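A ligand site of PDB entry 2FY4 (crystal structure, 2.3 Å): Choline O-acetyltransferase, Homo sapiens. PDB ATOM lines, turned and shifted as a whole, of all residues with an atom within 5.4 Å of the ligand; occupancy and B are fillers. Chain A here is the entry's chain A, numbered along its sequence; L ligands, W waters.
The backbone carbonyl oxygen (O) of Glu 434 sits at hydrogen-bond distance from the backbone NH (N) of Ile 449.
O of Gln 144 is in hydrogen-bond range of NH2 of Arg 440 (2.6 Å).
The side-chain hydroxyl of Tyr 561 lies within hydrogen-bond range of the side-chain carboxylate of Glu 434, 3.1 Å away.
The side-chain hydroxyl of Ser 409 lies within hydrogen-bond range of the backbone NH of Ala 412.
OD2 of Asp 411 lies close to OE2 of Glu 434 (2.5 Å).
The side-chain carboxylate of Asp 411 is in hydrogen-bond range of the side-chain amide nitrogen of Gln 538 (2.7 Å).
OD1 of Asp 411 lies within hydrogen-bond range of OH of Tyr 561, at 2.6 Å.
The side-chain amino group (NZ) of Lys 404 lies within salt-bridge range of an oxygen (O4) of the ligand, at 3.3 Å.
The backbone NH (N) of Asp 411 sits at hydrogen-bond distance from an oxygen (O9) of the ligand.
An oxygen (O11) of the ligand sits at hydrogen-bond distance from the backbone NH (N) of Gln 144 (2.7 Å).
The side-chain hydroxyl (OG) of Ser 409 lies within hydrogen-bond range of an oxygen (O9) of the ligand, 3.2 Å away.
N of Gly 329 sits close to S1 of the ligand, at 3.5 Å.
The side-chain amide nitrogen (NE2) of Gln 144 is in hydrogen-bond range of an oxygen (O8) of the ligand, 2.7 Å away.
A sulfur (S1) of the ligand sits close to the side-chain carboxylate of Asp 328, at 3.8 Å.
An oxygen (O4) of the ligand lies within salt-bridge range of the side-chain amino group of Lys 400, 3.8 Å away.
O of Gln 538 sits at hydrogen-bond distance from N7 of the ligand, 3.1 Å away.
An oxygen (O15) of the ligand sits at hydrogen-bond distance from the backbone NH (N) of Ser 437, at 2.7 Å.
The backbone carbonyl oxygen of Lys 407 is in hydrogen-bond range of a nitrogen (N3) of the ligand, at 3.3 Å.
The backbone nitrogen (N) of Pro 410 sits close to an oxygen (O9) of the ligand (3.0 Å).
CA of Gly 143 touches O11 of the ligand, at 3.4 Å.
His 324 touches the ligand (CE1 to S1, 3.7 Å).
Ile 330 touches the ligand.
N of Cys 408 touches N1 of the ligand, at 3.6 Å.
Glu 434 touches the ligand (OE2 to C14, 3.7 Å).
Ser 435 touches the ligand.
Ala 436 touches the ligand (C to O15, 3.6 Å).
CD1 of Ile 449 touches C13 of the ligand, at 3.6 Å.
Thr 490 touches the ligand (CG2 to C13, 3.4 Å).
Ile 494 touches the ligand.
Hydrophobic or aromatic side chains that line the ligand: His 324, Ile 330, Pro 410, Ile 449 and Ile 494.
Within 4 Å of the ligand: Gly 143, Gln 144, His 324, Asp 328, Gly 329, Ile 330, Lys 400, Lys 404, Lys 407, Cys 408, Ser 409, Pro 410, Asp 411, Glu 434, Ser 435, Ala 436, Ser 437, Ile 449, Thr 490, Ile 494 and Gln 538.
Along chain A the residues within 4 Å of the ligand span positions 143 to 538.
Water W6 lies within hydrogen-bond range of O14 of the ligand (2.9 Å), O of Ser 437 (2.9 Å) and NH1 of Arg 440 (3.1 Å).
Water W4 lies within hydrogen-bond range of OE1 of Gln 538 and N6 of the ligand.
Water W3 bridges OG of Ser 537 (3.0 Å) and S1 of the ligand (3.2 Å).
Water W7 lies within hydrogen-bond range of N of Gly 329 (3.1 Å), NE2 of His 324 (3.1 Å) and S1 of the ligand (3.4 Å).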
ATOM      1  N   LYS A 142      25.262  30.713 -10.832  1.00  0.00           N
ATOM      2  CA  LYS A 142      26.625  30.250 -10.849  1.00  0.00           C
ATOM      3  C   LYS A 142      26.636  28.766 -10.460  1.00  0.00           C
ATOM      4  O   LYS A 142      25.674  28.275  -9.865  1.00  0.00           O
ATOM      5  CB  LYS A 142      27.492  31.123  -9.944  1.00  0.00           C
ATOM      6  CG  LYS A 142      26.943  31.380  -8.566  1.00  0.00           C
ATOM      7  CD  LYS A 142      27.846  32.335  -7.841  1.00  0.00           C
ATOM      8  CE  LYS A 142      27.541  32.364  -6.363  1.00  0.00           C
ATOM      9  NZ  LYS A 142      28.571  33.180  -5.666  1.00  0.00           N
ATOM     10  N   GLY A 143      27.687  28.034 -10.830  1.00  0.00           N
ATOM     11  CA  GLY A 143      27.722  26.604 -10.561  1.00  0.00           C
ATOM     12  C   GLY A 143      27.037  25.898 -11.733  1.00  0.00           C
ATOM     13  O   GLY A 143      27.450  26.069 -12.895  1.00  0.00           O
ATOM     14  N   GLN A 144      26.001  25.106 -11.434  1.00  0.00           N
ATOM     15  CA  GLN A 144      25.255  24.406 -12.491  1.00  0.00           C
ATOM     16  C   GLN A 144      24.425  25.412 -13.310  1.00  0.00           C
ATOM     17  O   GLN A 144      23.634  26.148 -12.721  1.00  0.00           O
ATOM     18  CB  GLN A 144      24.285  23.358 -11.885  1.00  0.00           C
ATOM     19  CG  GLN A 144      24.901  22.289 -10.994  1.00  0.00           C
ATOM     20  CD  GLN A 144      25.586  21.143 -11.758  1.00  0.00           C
ATOM     21  OE1 GLN A 144      25.192  20.760 -12.857  1.00  0.00           O
ATOM     22  NE2 GLN A 144      26.604  20.580 -11.157  1.00  0.00           N
ATOM     23  N   HIS A 324      12.712  31.047   8.713  1.00  0.00           N
ATOM     24  CA  HIS A 324      12.773  30.481   7.378  1.00  0.00           C
ATOM     25  C   HIS A 324      11.715  30.834   6.329  1.00  0.00           C
ATOM     26  O   HIS A 324      12.030  30.956   5.141  1.00  0.00           O
ATOM     27  CB  HIS A 324      12.738  28.982   7.497  1.00  0.00           C
ATOM     28  CG  HIS A 324      13.626  28.301   6.464  1.00  0.00           C
ATOM     29  ND1 HIS A 324      13.621  28.595   5.115  1.00  0.00           N
ATOM     30  CD2 HIS A 324      14.551  27.332   6.645  1.00  0.00           C
ATOM     31  CE1 HIS A 324      14.512  27.830   4.503  1.00  0.00           C
ATOM     32  NE2 HIS A 324      15.087  27.058   5.401  1.00  0.00           N
ATOM     33  N   ASP A 328      15.249  32.106   1.727  1.00  0.00           N
ATOM     34  CA  ASP A 328      16.177  31.003   1.958  1.00  0.00           C
ATOM     35  C   ASP A 328      17.605  31.450   2.279  1.00  0.00           C
ATOM     36  O   ASP A 328      17.958  32.623   2.130  1.00  0.00           O
ATOM     37  CB  ASP A 328      16.127  30.062   0.756  1.00  0.00           C
ATOM     38  CG  ASP A 328      14.718  29.488   0.541  1.00  0.00           C
ATOM     39  OD1 ASP A 328      14.141  28.971   1.519  1.00  0.00           O
ATOM     40  OD2 ASP A 328      14.237  29.551  -0.603  1.00  0.00           O
ATOM     41  N   GLY A 329      18.414  30.493   2.711  1.00  0.00           N
ATOM     42  CA  GLY A 329      19.792  30.740   3.136  1.00  0.00           C
ATOM     43  C   GLY A 329      20.757  31.457   2.175  1.00  0.00           C
ATOM     44  O   GLY A 329      21.665  32.167   2.641  1.00  0.00           O
ATOM     45  N   ILE A 330      20.609  31.310   0.868  1.00  0.00           N
ATOM     46  CA  ILE A 330      21.543  31.967  -0.031  1.00  0.00           C
ATOM     47  C   ILE A 330      21.367  33.470   0.059  1.00  0.00           C
ATOM     48  O   ILE A 330      22.328  34.208   0.243  1.00  0.00           O
ATOM     49  CB  ILE A 330      21.348  31.523  -1.502  1.00  0.00           C
ATOM     50  CG1 ILE A 330      21.409  29.997  -1.600  1.00  0.00           C
ATOM     51  CG2 ILE A 330      22.384  32.174  -2.378  1.00  0.00           C
ATOM     52  CD1 ILE A 330      22.668  29.399  -1.001  1.00  0.00           C
ATOM     53  N   LYS A 400      36.668  21.279  -2.774  1.00  0.00           N
ATOM     54  CA  LYS A 400      36.256  21.390  -4.172  1.00  0.00           C
ATOM     55  C   LYS A 400      37.394  21.150  -5.165  1.00  0.00           C
ATOM     56  O   LYS A 400      37.223  20.427  -6.154  1.00  0.00           O
ATOM     57  CB  LYS A 400      35.648  22.776  -4.415  1.00  0.00           C
ATOM     58  CG  LYS A 400      34.454  23.069  -3.528  1.00  0.00           C
ATOM     59  CD  LYS A 400      34.160  24.564  -3.451  1.00  0.00           C
ATOM     60  CE  LYS A 400      33.762  25.134  -4.793  1.00  0.00           C
ATOM     61  NZ  LYS A 400      33.620  26.608  -4.740  1.00  0.00           N
ATOM     62  N   LYS A 404      36.985  18.587  -8.228  1.00  0.00           N
ATOM     63  CA  LYS A 404      36.907  19.006  -9.620  1.00  0.00           C
ATOM     64  C   LYS A 404      37.953  18.254 -10.449  1.00  0.00           C
ATOM     65  O   LYS A 404      37.742  18.001 -11.637  1.00  0.00           O
ATOM     66  CB  LYS A 404      37.162  20.512  -9.737  1.00  0.00           C
ATOM     67  CG  LYS A 404      36.051  21.382  -9.177  1.00  0.00           C
ATOM     68  CD  LYS A 404      36.460  22.837  -9.277  1.00  0.00           C
ATOM     69  CE  LYS A 404      35.336  23.767  -8.891  1.00  0.00           C
ATOM     70  NZ  LYS A 404      35.806  25.183  -8.937  1.00  0.00           N
ATOM     71  N   LYS A 407      36.757  15.383 -12.191  1.00  0.00           N
ATOM     72  CA  LYS A 407      35.720  15.684 -13.179  1.00  0.00           C
ATOM     73  C   LYS A 407      34.342  15.467 -12.549  1.00  0.00           C
ATOM     74  O   LYS A 407      33.432  14.934 -13.159  1.00  0.00           O
ATOM     75  CB  LYS A 407      35.886  14.799 -14.413  1.00  0.00           C
ATOM     76  CG  LYS A 407      37.206  14.989 -15.142  1.00  0.00           C
ATOM     77  CD  LYS A 407      37.242  14.188 -16.443  1.00  0.00           C
ATOM     78  CE  LYS A 407      37.104  12.700 -16.169  1.00  0.00           C
ATOM     79  NZ  LYS A 407      36.990  11.893 -17.414  1.00  0.00           N
ATOM     80  N   CYS A 408      34.226  15.916 -11.287  1.00  0.00           N
ATOM     81  CA  CYS A 408      33.001  15.720 -10.557  1.00  0.00           C
ATOM     82  C   CYS A 408      32.450  17.013  -9.939  1.00  0.00           C
ATOM     83  O   CYS A 408      33.206  17.900  -9.523  1.00  0.00           O
ATOM     84  CB  CYS A 408      33.221  14.690  -9.437  1.00  0.00           C
ATOM     85  SG  CYS A 408      33.429  12.978 -10.009  1.00  0.00           S
ATOM     86  N   SER A 409      31.141  17.068  -9.905  1.00  0.00           N
ATOM     87  CA  SER A 409      30.480  18.213  -9.310  1.00  0.00           C
ATOM     88  C   SER A 409      30.717  18.163  -7.780  1.00  0.00           C
ATOM     89  O   SER A 409      30.420  17.125  -7.191  1.00  0.00           O
ATOM     90  CB  SER A 409      28.982  18.232  -9.649  1.00  0.00           C
ATOM     91  OG  SER A 409      28.204  18.621  -8.526  1.00  0.00           O
ATOM     92  N   PRO A 410      31.272  19.176  -7.088  1.00  0.00           N
ATOM     93  CA  PRO A 410      31.490  19.007  -5.655  1.00  0.00           C
ATOM     94  C   PRO A 410      30.190  18.585  -4.952  1.00  0.00           C
ATOM     95  O   PRO A 410      30.126  17.556  -4.272  1.00  0.00           O
ATOM     96  CB  PRO A 410      32.077  20.356  -5.239  1.00  0.00           C
ATOM     97  CG  PRO A 410      32.563  20.970  -6.511  1.00  0.00           C
ATOM     98  CD  PRO A 410      31.682  20.479  -7.620  1.00  0.00           C
ATOM     99  N   ASP A 411      29.149  19.424  -5.170  1.00  0.00           N
ATOM    100  CA  ASP A 411      27.865  19.191  -4.542  1.00  0.00           C
ATOM    101  C   ASP A 411      27.425  17.757  -4.723  1.00  0.00           C
ATOM    102  O   ASP A 411      27.053  17.090  -3.757  1.00  0.00           O
ATOM    103  CB  ASP A 411      26.800  20.137  -5.106  1.00  0.00           C
ATOM    104  CG  ASP A 411      25.548  20.093  -4.247  1.00  0.00           C
ATOM    105  OD1 ASP A 411      25.576  20.672  -3.143  1.00  0.00           O
ATOM    106  OD2 ASP A 411      24.544  19.466  -4.665  1.00  0.00           O
ATOM    107  N   ALA A 412      27.439  17.256  -5.954  1.00  0.00           N
ATOM    108  CA  ALA A 412      27.045  15.878  -6.215  1.00  0.00           C
ATOM    109  C   ALA A 412      27.925  14.898  -5.435  1.00  0.00           C
ATOM    110  O   ALA A 412      27.431  13.958  -4.816  1.00  0.00           O
ATOM    111  CB  ALA A 412      27.126  15.580  -7.704  1.00  0.00           C
ATOM    112  N   GLU A 434      17.399  17.640  -0.527  1.00  0.00           N
ATOM    113  CA  GLU A 434      18.455  18.613  -0.745  1.00  0.00           C
ATOM    114  C   GLU A 434      17.830  19.824  -1.415  1.00  0.00           C
ATOM    115  O   GLU A 434      17.200  19.711  -2.469  1.00  0.00           O
ATOM    116  CB  GLU A 434      19.600  18.106  -1.639  1.00  0.00           C
ATOM    117  CG  GLU A 434      20.589  19.249  -1.904  1.00  0.00           C
ATOM    118  CD  GLU A 434      21.708  18.905  -2.884  1.00  0.00           C
ATOM    119  OE1 GLU A 434      21.679  17.811  -3.473  1.00  0.00           O
ATOM    120  OE2 GLU A 434      22.616  19.752  -3.069  1.00  0.00           O
ATOM    121  N   SER A 435      17.996  20.974  -0.774  1.00  0.00           N
ATOM    122  CA  SER A 435      17.457  22.215  -1.284  1.00  0.00           C
ATOM    123  C   SER A 435      18.066  22.528  -2.637  1.00  0.00           C
ATOM    124  O   SER A 435      19.293  22.564  -2.785  1.00  0.00           O
ATOM    125  CB  SER A 435      17.787  23.371  -0.322  1.00  0.00           C
ATOM    126  OG  SER A 435      17.399  23.038   0.996  1.00  0.00           O
ATOM    127  N   ALA A 436      17.212  22.731  -3.627  1.00  0.00           N
ATOM    128  CA  ALA A 436      17.667  23.069  -4.965  1.00  0.00           C
ATOM    129  C   ALA A 436      16.998  24.396  -5.287  1.00  0.00           C
ATOM    130  O   ALA A 436      15.772  24.483  -5.357  1.00  0.00           O
ATOM    131  CB  ALA A 436      17.250  21.995  -5.951  1.00  0.00           C
ATOM    132  N   SER A 437      17.800  25.446  -5.467  1.00  0.00           N
ATOM    133  CA  SER A 437      17.237  26.750  -5.753  1.00  0.00           C
ATOM    134  C   SER A 437      16.604  26.831  -7.129  1.00  0.00           C
ATOM    135  O   SER A 437      17.195  26.412  -8.113  1.00  0.00           O
ATOM    136  CB  SER A 437      18.298  27.836  -5.641  1.00  0.00           C
ATOM    137  OG  SER A 437      17.759  29.096  -6.002  1.00  0.00           O
ATOM    138  N   ARG A 440      15.628  30.818 -10.670  1.00  0.00           N
ATOM    139  CA  ARG A 440      15.717  31.159 -12.084  1.00  0.00           C
ATOM    140  C   ARG A 440      14.323  31.570 -12.545  1.00  0.00           C
ATOM    141  O   ARG A 440      14.168  32.174 -13.614  1.00  0.00           O
ATOM    142  CB  ARG A 440      16.171  29.955 -12.906  1.00  0.00           C
ATOM    143  CG  ARG A 440      17.626  29.578 -12.692  1.00  0.00           C
ATOM    144  CD  ARG A 440      18.031  28.352 -13.508  1.00  0.00           C
ATOM    145  NE  ARG A 440      19.484  28.129 -13.485  1.00  0.00           N
ATOM    146  CZ  ARG A 440      20.187  27.831 -12.387  1.00  0.00           C
ATOM    147  NH1 ARG A 440      19.599  27.706 -11.205  1.00  0.00           N
ATOM    148  NH2 ARG A 440      21.492  27.654 -12.467  1.00  0.00           N
ATOM    149  N   VAL A 446      12.581  27.011  -3.714  1.00  0.00           N
ATOM    150  CA  VAL A 446      13.377  25.804  -3.931  1.00  0.00           C
ATOM    151  C   VAL A 446      12.501  24.605  -4.227  1.00  0.00           C
ATOM    152  O   VAL A 446      11.306  24.604  -3.921  1.00  0.00           O
ATOM    153  CB  VAL A 446      14.226  25.419  -2.714  1.00  0.00           C
ATOM    154  CG1 VAL A 446      15.048  26.607  -2.244  1.00  0.00           C
ATOM    155  CG2 VAL A 446      13.323  24.902  -1.596  1.00  0.00           C
ATOM    156  N   ILE A 449      15.905  17.865  -4.481  1.00  0.00           N
ATOM    157  CA  ILE A 449      16.825  16.967  -5.167  1.00  0.00           C
ATOM    158  C   ILE A 449      16.814  15.706  -4.327  1.00  0.00           C
ATOM    159  O   ILE A 449      17.315  15.738  -3.201  1.00  0.00           O
ATOM    160  CB  ILE A 449      18.250  17.548  -5.255  1.00  0.00           C
ATOM    161  CG1 ILE A 449      18.300  18.752  -6.193  1.00  0.00           C
ATOM    162  CG2 ILE A 449      19.223  16.472  -5.732  1.00  0.00           C
ATOM    163  CD1 ILE A 449      19.623  19.484  -6.163  1.00  0.00           C
ATOM    164  N   THR A 490      20.092  16.928 -10.120  1.00  0.00           N
ATOM    165  CA  THR A 490      20.332  18.305  -9.740  1.00  0.00           C
ATOM    166  C   THR A 490      19.900  19.201 -10.902  1.00  0.00           C
ATOM    167  O   THR A 490      19.112  20.140 -10.725  1.00  0.00           O
ATOM    168  CB  THR A 490      21.828  18.501  -9.389  1.00  0.00           C
ATOM    169  OG1 THR A 490      22.155  17.686  -8.246  1.00  0.00           O
ATOM    170  CG2 THR A 490      22.140  19.946  -9.069  1.00  0.00           C
ATOM    171  N   ILE A 494      16.830  22.061 -10.562  1.00  0.00           N
ATOM    172  CA  ILE A 494      17.045  23.492 -10.726  1.00  0.00           C
ATOM    173  C   ILE A 494      16.420  24.091 -11.981  1.00  0.00           C
ATOM    174  O   ILE A 494      16.352  25.322 -12.127  1.00  0.00           O
ATOM    175  CB  ILE A 494      18.540  23.856 -10.664  1.00  0.00           C
ATOM    176  CG1 ILE A 494      19.295  23.209 -11.823  1.00  0.00           C
ATOM    177  CG2 ILE A 494      19.114  23.402  -9.333  1.00  0.00           C
ATOM    178  CD1 ILE A 494      20.791  23.505 -11.805  1.00  0.00           C
ATOM    179  N   SER A 537      21.421  20.550   2.633  1.00  0.00           N
ATOM    180  CA  SER A 537      21.529  21.747   1.823  1.00  0.00           C
ATOM    181  C   SER A 537      22.951  22.288   1.821  1.00  0.00           C
ATOM    182  O   SER A 537      23.693  22.122   2.796  1.00  0.00           O
ATOM    183  CB  SER A 537      20.596  22.849   2.334  1.00  0.00           C
ATOM    184  OG  SER A 537      21.117  23.426   3.520  1.00  0.00           O
ATOM    185  N   GLN A 538      23.319  22.927   0.727  1.00  0.00           N
ATOM    186  CA  GLN A 538      24.629  23.540   0.610  1.00  0.00           C
ATOM    187  C   GLN A 538      24.429  25.039   0.833  1.00  0.00           C
ATOM    188  O   GLN A 538      23.594  25.664   0.191  1.00  0.00           O
ATOM    189  CB  GLN A 538      25.232  23.332  -0.785  1.00  0.00           C
ATOM    190  CG  GLN A 538      26.627  23.933  -0.935  1.00  0.00           C
ATOM    191  CD  GLN A 538      27.045  24.087  -2.372  1.00  0.00           C
ATOM    192  OE1 GLN A 538      27.371  25.188  -2.813  1.00  0.00           O
ATOM    193  NE2 GLN A 538      27.046  22.985  -3.114  1.00  0.00           N
ATOM    194  N   VAL A 539      25.164  25.602   1.781  1.00  0.00           N
ATOM    195  CA  VAL A 539      25.089  27.035   2.059  1.00  0.00           C
ATOM    196  C   VAL A 539      26.536  27.489   2.052  1.00  0.00           C
ATOM    197  O   VAL A 539      27.200  27.528   3.094  1.00  0.00           O
ATOM    198  CB  VAL A 539      24.450  27.366   3.432  1.00  0.00           C
ATOM    199  CG1 VAL A 539      24.488  28.869   3.684  1.00  0.00           C
ATOM    200  CG2 VAL A 539      22.992  26.889   3.466  1.00  0.00           C
ATOM    201  N   TYR A 561      26.202  21.858   4.552  1.00  0.00           N
ATOM    202  CA  TYR A 561      27.639  21.927   4.305  1.00  0.00           C
ATOM    203  C   TYR A 561      28.101  23.160   3.537  1.00  0.00           C
ATOM    204  O   TYR A 561      27.351  23.773   2.792  1.00  0.00           O
ATOM    205  CB  TYR A 561      28.094  20.657   3.578  1.00  0.00           C
ATOM    206  CG  TYR A 561      27.257  20.321   2.368  1.00  0.00           C
ATOM    207  CD1 TYR A 561      26.039  19.671   2.505  1.00  0.00           C
ATOM    208  CD2 TYR A 561      27.674  20.679   1.087  1.00  0.00           C
ATOM    209  CE1 TYR A 561      25.251  19.380   1.405  1.00  0.00           C
ATOM    210  CE2 TYR A 561      26.893  20.384  -0.029  1.00  0.00           C
ATOM    211  CZ  TYR A 561      25.685  19.739   0.143  1.00  0.00           C
ATOM    212  OH  TYR A 561      24.883  19.483  -0.960  1.00  0.00           O
HETATM  213  N1  LIG L   1      33.842  18.896 -13.355  1.00  0.00           N
HETATM  214  C1  LIG L   1      34.541  19.931 -12.919  1.00  0.00           C
HETATM  215  N2  LIG L   1      33.963  20.957 -12.316  1.00  0.00           N
HETATM  216  C2  LIG L   1      32.634  20.977 -12.108  1.00  0.00           C
HETATM  217  C3  LIG L   1      31.861  19.909 -12.559  1.00  0.00           C
HETATM  218  C4  LIG L   1      32.506  18.847 -13.189  1.00  0.00           C
HETATM  219  N3  LIG L   1      31.806  17.799 -13.596  1.00  0.00           N
HETATM  220  N4  LIG L   1      30.603  20.164 -12.225  1.00  0.00           N
HETATM  221  C5  LIG L   1      30.579  21.326 -11.586  1.00  0.00           C
HETATM  222  N5  LIG L   1      31.814  21.837 -11.519  1.00  0.00           N
HETATM  223  C6  LIG L   1      32.180  23.131 -10.907  1.00  0.00           C
HETATM  224  C7  LIG L   1      31.386  24.299 -11.486  1.00  0.00           C
HETATM  225  O1  LIG L   1      31.979  24.715 -12.726  1.00  0.00           O
HETATM  226  C8  LIG L   1      31.619  25.333 -10.390  1.00  0.00           C
HETATM  227  O2  LIG L   1      32.967  25.819 -10.406  1.00  0.00           O
HETATM  228  P1  LIG L   1      33.156  27.376 -10.050  1.00  0.00           P
HETATM  229  O3  LIG L   1      31.953  28.142 -10.447  1.00  0.00           O
HETATM  230  O4  LIG L   1      33.477  27.489  -8.479  1.00  0.00           O
HETATM  231  O5  LIG L   1      34.492  27.785 -10.851  1.00  0.00           O
HETATM  232  C9  LIG L   1      31.425  24.480  -9.143  1.00  0.00           C
HETATM  233  O6  LIG L   1      32.005  23.196  -9.477  1.00  0.00           O
HETATM  234  C10 LIG L   1      29.924  24.257  -8.938  1.00  0.00           C
HETATM  235  O7  LIG L   1      29.889  23.166  -8.031  1.00  0.00           O
HETATM  236  P2  LIG L   1      28.621  22.198  -7.892  1.00  0.00           P
HETATM  237  O8  LIG L   1      28.059  21.742  -9.192  1.00  0.00           O
HETATM  238  O9  LIG L   1      29.058  21.215  -6.878  1.00  0.00           O
HETATM  239  O10 LIG L   1      27.691  23.196  -7.039  1.00  0.00           O
HETATM  240  P3  LIG L   1      26.493  24.169  -7.476  1.00  0.00           P
HETATM  241  O11 LIG L   1      26.145  24.096  -8.915  1.00  0.00           O
HETATM  242  O12 LIG L   1      26.949  25.443  -6.880  1.00  0.00           O
HETATM  243  O13 LIG L   1      25.340  23.577  -6.521  1.00  0.00           O
HETATM  244  C11 LIG L   1      23.030  23.170  -6.167  1.00  0.00           C
HETATM  245  C12 LIG L   1      24.271  22.743  -6.960  1.00  0.00           C
HETATM  246  C13 LIG L   1      21.835  22.300  -6.582  1.00  0.00           C
HETATM  247  C14 LIG L   1      23.288  22.991  -4.671  1.00  0.00           C
HETATM  248  C15 LIG L   1      22.771  24.645  -6.480  1.00  0.00           C
HETATM  249  O14 LIG L   1      22.327  24.763  -7.842  1.00  0.00           O
HETATM  250  C16 LIG L   1      21.700  25.270  -5.588  1.00  0.00           C
HETATM  251  O15 LIG L   1      20.507  25.200  -5.872  1.00  0.00           O
HETATM  252  N6  LIG L   1      22.180  25.919  -4.527  1.00  0.00           N
HETATM  253  C17 LIG L   1      21.282  26.580  -3.570  1.00  0.00           C
HETATM  254  C18 LIG L   1      21.320  25.889  -2.204  1.00  0.00           C
HETATM  255  C19 LIG L   1      20.291  26.571  -1.298  1.00  0.00           C
HETATM  256  O16 LIG L   1      19.210  26.929  -1.735  1.00  0.00           O
HETATM  257  N7  LIG L   1      20.686  26.754  -0.030  1.00  0.00           N
HETATM  258  C20 LIG L   1      19.796  27.384   0.945  1.00  0.00           C
HETATM  259  C21 LIG L   1      18.648  26.422   1.245  1.00  0.00           C
HETATM  260  S1  LIG L   1      17.387  27.210   2.312  1.00  0.00           S
HETATM  261  O   HOH W   1      18.364  29.816  -2.610  1.00  0.00           O
HETATM  262  O   HOH W   2      36.219  22.772 -12.724  1.00  0.00           O
HETATM  263  O   HOH W   3      19.397  25.736   4.245  1.00  0.00           O
HETATM  264  O   HOH W   4      25.219  26.661  -4.227  1.00  0.00           O
HETATM  265  O   HOH W   5      21.788  28.299  -7.276  1.00  0.00           O
HETATM  266  O   HOH W   6      20.068  26.385  -8.466  1.00  0.00           O
HETATM  267  O   HOH W   7      17.618  28.896   5.263  1.00  0.00           O
